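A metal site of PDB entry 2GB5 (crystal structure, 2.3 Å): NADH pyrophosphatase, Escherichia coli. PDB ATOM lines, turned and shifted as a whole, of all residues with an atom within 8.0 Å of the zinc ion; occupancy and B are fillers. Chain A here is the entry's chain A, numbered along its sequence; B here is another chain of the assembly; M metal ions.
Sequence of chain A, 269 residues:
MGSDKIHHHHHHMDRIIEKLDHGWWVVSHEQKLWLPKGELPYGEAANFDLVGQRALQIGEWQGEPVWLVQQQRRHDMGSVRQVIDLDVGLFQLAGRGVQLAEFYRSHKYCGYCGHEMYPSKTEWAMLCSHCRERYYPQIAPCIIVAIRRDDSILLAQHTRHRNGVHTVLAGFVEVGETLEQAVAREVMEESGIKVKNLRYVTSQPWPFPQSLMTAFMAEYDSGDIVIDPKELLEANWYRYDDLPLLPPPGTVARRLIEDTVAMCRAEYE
The backbone NH of His 115 sits close to the side-chain sulfur of Cys 113 (3.6 Å).
The side-chain sulfur of Cys 131 lies close to the backbone NH of Glu 133 (3.6 Å).
The side-chain sulfur (SG) of Cys 128 lies close to the backbone NH (N) of His 130.
The backbone carbonyl oxygen of His 115 is in hydrogen-bond range of the backbone NH of Cys 110 (2.7 Å).
The side-chain sulfur (SG) of Cys 110 lies close to the backbone NH (N) of Tyr 112.
Along chain A the residues within 4 Å of the zinc ion span positions 110 to 131.
The zinc ion is bound by the side-chain sulfur (SG) of Cys 113 (2.3 Å), the side-chain sulfur (SG) of Cys 131 (2.3 Å), the side-chain sulfur (SG) of Cys 128 (2.4 Å) and the side-chain sulfur (SG) of Cys 110 (2.5 Å).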
ATOM      1  N   TYR A 109      14.366 -16.979  19.442  1.00  0.00           N
ATOM      2  CA  TYR A 109      13.239 -17.458  20.191  1.00  0.00           C
ATOM      3  C   TYR A 109      13.714 -18.134  21.457  1.00  0.00           C
ATOM      4  O   TYR A 109      14.821 -18.658  21.520  1.00  0.00           O
ATOM      5  CB  TYR A 109      12.434 -18.440  19.370  1.00  0.00           C
ATOM      6  CG  TYR A 109      11.918 -17.856  18.101  1.00  0.00           C
ATOM      7  CD1 TYR A 109      10.705 -17.150  18.080  1.00  0.00           C
ATOM      8  CD2 TYR A 109      12.636 -17.982  16.914  1.00  0.00           C
ATOM      9  CE1 TYR A 109      10.226 -16.615  16.919  1.00  0.00           C
ATOM     10  CE2 TYR A 109      12.172 -17.431  15.746  1.00  0.00           C
ATOM     11  CZ  TYR A 109      10.967 -16.757  15.756  1.00  0.00           C
ATOM     12  OH  TYR A 109      10.479 -16.226  14.584  1.00  0.00           O
ATOM     13  N   CYS A 110      12.874 -18.078  22.466  1.00  0.00           N
ATOM     14  CA  CYS A 110      13.116 -18.711  23.733  1.00  0.00           C
ATOM     15  C   CYS A 110      12.810 -20.182  23.624  1.00  0.00           C
ATOM     16  O   CYS A 110      11.716 -20.559  23.249  1.00  0.00           O
ATOM     17  CB  CYS A 110      12.246 -18.082  24.811  1.00  0.00           C
ATOM     18  SG  CYS A 110      12.372 -18.938  26.398  1.00  0.00           S
ATOM     19  N   GLY A 111      13.781 -21.033  23.937  1.00  0.00           N
ATOM     20  CA  GLY A 111      13.603 -22.475  23.868  1.00  0.00           C
ATOM     21  C   GLY A 111      12.719 -23.060  24.962  1.00  0.00           C
ATOM     22  O   GLY A 111      12.269 -24.183  24.844  1.00  0.00           O
ATOM     23  N   TYR A 112      12.488 -22.296  26.016  1.00  0.00           N
ATOM     24  CA  TYR A 112      11.559 -22.722  27.057  1.00  0.00           C
ATOM     25  C   TYR A 112      10.106 -22.578  26.626  1.00  0.00           C
ATOM     26  O   TYR A 112       9.323 -23.544  26.709  1.00  0.00           O
ATOM     27  CB  TYR A 112      11.782 -21.902  28.339  1.00  0.00           C
ATOM     28  CG  TYR A 112      13.021 -22.247  29.094  1.00  0.00           C
ATOM     29  CD1 TYR A 112      13.001 -23.220  30.083  1.00  0.00           C
ATOM     30  CD2 TYR A 112      14.213 -21.572  28.870  1.00  0.00           C
ATOM     31  CE1 TYR A 112      14.147 -23.544  30.821  1.00  0.00           C
ATOM     32  CE2 TYR A 112      15.379 -21.885  29.588  1.00  0.00           C
ATOM     33  CZ  TYR A 112      15.323 -22.862  30.579  1.00  0.00           C
ATOM     34  OH  TYR A 112      16.437 -23.206  31.292  1.00  0.00           O
ATOM     35  N   CYS A 113       9.754 -21.374  26.178  1.00  0.00           N
ATOM     36  CA  CYS A 113       8.373 -21.018  25.836  1.00  0.00           C
ATOM     37  C   CYS A 113       8.128 -20.579  24.375  1.00  0.00           C
ATOM     38  O   CYS A 113       6.981 -20.366  23.971  1.00  0.00           O
ATOM     39  CB  CYS A 113       7.908 -19.897  26.753  1.00  0.00           C
ATOM     40  SG  CYS A 113       8.497 -18.274  26.276  1.00  0.00           S
ATOM     41  N   GLY A 114       9.180 -20.443  23.583  1.00  0.00           N
ATOM     42  CA  GLY A 114       9.027 -20.185  22.155  1.00  0.00           C
ATOM     43  C   GLY A 114       8.773 -18.746  21.757  1.00  0.00           C
ATOM     44  O   GLY A 114       8.639 -18.462  20.565  1.00  0.00           O
ATOM     45  N   HIS A 115       8.707 -17.832  22.726  1.00  0.00           N
ATOM     46  CA  HIS A 115       8.470 -16.421  22.444  1.00  0.00           C
ATOM     47  C   HIS A 115       9.765 -15.757  22.050  1.00  0.00           C
ATOM     48  O   HIS A 115      10.865 -16.280  22.314  1.00  0.00           O
ATOM     49  CB  HIS A 115       7.861 -15.688  23.646  1.00  0.00           C
ATOM     50  CG  HIS A 115       6.413 -15.989  23.857  1.00  0.00           C
ATOM     51  ND1 HIS A 115       5.428 -15.025  23.768  1.00  0.00           N
ATOM     52  CD2 HIS A 115       5.768 -17.145  24.144  1.00  0.00           C
ATOM     53  CE1 HIS A 115       4.250 -15.574  23.987  1.00  0.00           C
ATOM     54  NE2 HIS A 115       4.424 -16.868  24.215  1.00  0.00           N
ATOM     55  N   GLU A 116       9.651 -14.585  21.435  1.00  0.00           N
ATOM     56  CA  GLU A 116      10.809 -13.838  20.973  1.00  0.00           C
ATOM     57  C   GLU A 116      11.615 -13.282  22.117  1.00  0.00           C
ATOM     58  O   GLU A 116      11.053 -12.867  23.126  1.00  0.00           O
ATOM     59  CB  GLU A 116      10.403 -12.709  20.035  1.00  0.00           C
ATOM     60  CG  GLU A 116       9.799 -13.231  18.759  1.00  0.00           C
ATOM     61  CD  GLU A 116       9.412 -12.123  17.813  1.00  0.00           C
ATOM     62  OE1 GLU A 116      10.007 -11.030  17.910  1.00  0.00           O
ATOM     63  OE2 GLU A 116       8.519 -12.364  16.959  1.00  0.00           O
ATOM     64  N   MET A 117      12.936 -13.276  21.944  1.00  0.00           N
ATOM     65  CA  MET A 117      13.853 -12.832  22.982  1.00  0.00           C
ATOM     66  C   MET A 117      14.451 -11.494  22.618  1.00  0.00           C
ATOM     67  O   MET A 117      14.433 -11.104  21.459  1.00  0.00           O
ATOM     68  CB  MET A 117      14.990 -13.835  23.131  1.00  0.00           C
ATOM     69  CG  MET A 117      14.519 -15.199  23.498  1.00  0.00           C
ATOM     70  SD  MET A 117      15.857 -16.274  24.393  1.00  0.00           S
ATOM     71  CE  MET A 117      15.298 -16.036  26.292  1.00  0.00           C
ATOM     72  N   LEU A 127      17.287 -12.210  27.137  1.00  0.00           N
ATOM     73  CA  LEU A 127      16.122 -12.225  28.006  1.00  0.00           C
ATOM     74  C   LEU A 127      14.853 -12.491  27.176  1.00  0.00           C
ATOM     75  O   LEU A 127      14.796 -12.202  25.969  1.00  0.00           O
ATOM     76  CB  LEU A 127      16.000 -10.883  28.741  1.00  0.00           C
ATOM     77  CG  LEU A 127      17.264 -10.330  29.426  1.00  0.00           C
ATOM     78  CD1 LEU A 127      16.922  -9.064  30.209  1.00  0.00           C
ATOM     79  CD2 LEU A 127      17.939 -11.338  30.346  1.00  0.00           C
ATOM     80  N   CYS A 128      13.847 -13.049  27.828  1.00  0.00           N
ATOM     81  CA  CYS A 128      12.629 -13.403  27.135  1.00  0.00           C
ATOM     82  C   CYS A 128      11.541 -12.378  27.376  1.00  0.00           C
ATOM     83  O   CYS A 128      11.386 -11.856  28.477  1.00  0.00           O
ATOM     84  CB  CYS A 128      12.154 -14.766  27.597  1.00  0.00           C
ATOM     85  SG  CYS A 128      10.761 -15.366  26.657  1.00  0.00           S
ATOM     86  N   SER A 129      10.764 -12.121  26.325  1.00  0.00           N
ATOM     87  CA  SER A 129       9.623 -11.242  26.422  1.00  0.00           C
ATOM     88  C   SER A 129       8.418 -11.847  27.172  1.00  0.00           C
ATOM     89  O   SER A 129       7.558 -11.097  27.657  1.00  0.00           O
ATOM     90  CB  SER A 129       9.220 -10.795  25.009  1.00  0.00           C
ATOM     91  OG  SER A 129       8.714 -11.884  24.257  1.00  0.00           O
ATOM     92  N   HIS A 130       8.328 -13.177  27.275  1.00  0.00           N
ATOM     93  CA  HIS A 130       7.162 -13.832  27.881  1.00  0.00           C
ATOM     94  C   HIS A 130       7.441 -14.482  29.244  1.00  0.00           C
ATOM     95  O   HIS A 130       6.704 -14.252  30.181  1.00  0.00           O
ATOM     96  CB  HIS A 130       6.609 -14.889  26.932  1.00  0.00           C
ATOM     97  CG  HIS A 130       5.425 -15.620  27.475  1.00  0.00           C
ATOM     98  ND1 HIS A 130       4.173 -15.046  27.564  1.00  0.00           N
ATOM     99  CD2 HIS A 130       5.290 -16.887  27.936  1.00  0.00           C
ATOM    100  CE1 HIS A 130       3.318 -15.914  28.069  1.00  0.00           C
ATOM    101  NE2 HIS A 130       3.972 -17.046  28.304  1.00  0.00           N
ATOM    102  N   CYS A 131       8.492 -15.292  29.343  1.00  0.00           N
ATOM    103  CA  CYS A 131       8.854 -15.942  30.605  1.00  0.00           C
ATOM    104  C   CYS A 131      10.106 -15.290  31.258  1.00  0.00           C
ATOM    105  O   CYS A 131      10.634 -14.297  30.755  1.00  0.00           O
ATOM    106  CB  CYS A 131       9.031 -17.466  30.377  1.00  0.00           C
ATOM    107  SG  CYS A 131      10.607 -17.993  29.593  1.00  0.00           S
ATOM    108  N   ARG A 132      10.558 -15.847  32.373  1.00  0.00           N
ATOM    109  CA  ARG A 132      11.648 -15.295  33.167  1.00  0.00           C
ATOM    110  C   ARG A 132      13.015 -15.894  32.820  1.00  0.00           C
ATOM    111  O   ARG A 132      14.044 -15.490  33.376  1.00  0.00           O
ATOM    112  CB  ARG A 132      11.369 -15.523  34.672  1.00  0.00           C
ATOM    113  CG  ARG A 132      11.474 -16.989  35.158  1.00  0.00           C
ATOM    114  CD  ARG A 132      11.318 -17.098  36.678  1.00  0.00           C
ATOM    115  NE  ARG A 132      12.491 -16.569  37.395  1.00  0.00           N
ATOM    116  CZ  ARG A 132      12.648 -16.576  38.720  1.00  0.00           C
ATOM    117  NH1 ARG A 132      11.696 -17.084  39.518  1.00  0.00           N
ATOM    118  NH2 ARG A 132      13.745 -16.079  39.266  1.00  0.00           N
ATOM    119  N   GLU A 133      13.043 -16.853  31.914  1.00  0.00           N
ATOM    120  CA  GLU A 133      14.280 -17.539  31.604  1.00  0.00           C
ATOM    121  C   GLU A 133      15.215 -16.673  30.778  1.00  0.00           C
ATOM    122  O   GLU A 133      14.815 -15.666  30.180  1.00  0.00           O
ATOM    123  CB  GLU A 133      14.014 -18.859  30.888  1.00  0.00           C
ATOM    124  CG  GLU A 133      13.040 -19.757  31.635  1.00  0.00           C
ATOM    125  CD  GLU A 133      13.579 -20.270  32.955  1.00  0.00           C
ATOM    126  OE1 GLU A 133      14.802 -20.206  33.173  1.00  0.00           O
ATOM    127  OE2 GLU A 133      12.784 -20.760  33.745  1.00  0.00           O
ATOM    128  N   ARG A 134      16.470 -17.090  30.756  1.00  0.00           N
ATOM    129  CA  ARG A 134      17.493 -16.403  29.984  1.00  0.00           C
ATOM    130  C   ARG A 134      18.618 -17.359  29.646  1.00  0.00           C
ATOM    131  O   ARG A 134      18.722 -18.474  30.195  1.00  0.00           O
ATOM    132  CB  ARG A 134      18.036 -15.224  30.771  1.00  0.00           C
ATOM    133  CG  ARG A 134      18.802 -15.581  31.992  1.00  0.00           C
ATOM    134  CD  ARG A 134      19.222 -14.355  32.730  1.00  0.00           C
ATOM    135  NE  ARG A 134      18.096 -13.679  33.372  1.00  0.00           N
ATOM    136  CZ  ARG A 134      18.228 -12.624  34.178  1.00  0.00           C
ATOM    137  NH1 ARG A 134      19.425 -12.096  34.432  1.00  0.00           N
ATOM    138  NH2 ARG A 134      17.149 -12.080  34.725  1.00  0.00           N
ATOM    139  N   TYR A 135      19.453 -16.902  28.706  1.00  0.00           N
ATOM    140  CA  TYR A 135      20.605 -17.657  28.226  1.00  0.00           C
ATOM    141  C   TYR A 135      21.830 -16.762  28.126  1.00  0.00           C
ATOM    142  O   TYR A 135      21.708 -15.562  27.898  1.00  0.00           O
ATOM    143  CB  TYR A 135      20.334 -18.259  26.845  1.00  0.00           C
ATOM    144  CG  TYR A 135      19.156 -19.182  26.722  1.00  0.00           C
ATOM    145  CD1 TYR A 135      17.869 -18.666  26.514  1.00  0.00           C
ATOM    146  CD2 TYR A 135      19.309 -20.564  26.727  1.00  0.00           C
ATOM    147  CE1 TYR A 135      16.770 -19.505  26.358  1.00  0.00           C
ATOM    148  CE2 TYR A 135      18.187 -21.422  26.566  1.00  0.00           C
ATOM    149  CZ  TYR A 135      16.939 -20.878  26.374  1.00  0.00           C
ATOM    150  OH  TYR A 135      15.816 -21.674  26.232  1.00  0.00           O
ATOM    151  N   TYR B 109      11.509 -25.500  22.234  1.00  0.00           N
ATOM    152  CA  TYR B 109      11.487 -24.771  20.977  1.00  0.00           C
ATOM    153  C   TYR B 109      12.882 -24.393  20.542  1.00  0.00           C
ATOM    154  O   TYR B 109      13.779 -24.151  21.365  1.00  0.00           O
ATOM    155  CB  TYR B 109      10.689 -23.493  21.122  1.00  0.00           C
ATOM    156  CG  TYR B 109       9.270 -23.686  21.562  1.00  0.00           C
ATOM    157  CD1 TYR B 109       8.255 -23.921  20.626  1.00  0.00           C
ATOM    158  CD2 TYR B 109       8.933 -23.638  22.903  1.00  0.00           C
ATOM    159  CE1 TYR B 109       6.941 -24.075  21.026  1.00  0.00           C
ATOM    160  CE2 TYR B 109       7.620 -23.795  23.314  1.00  0.00           C
ATOM    161  CZ  TYR B 109       6.627 -24.006  22.361  1.00  0.00           C
ATOM    162  OH  TYR B 109       5.356 -24.184  22.783  1.00  0.00           O
HETATM  163 ZN    ZN M   1      10.475 -17.649  27.278  1.00  0.00          ZN
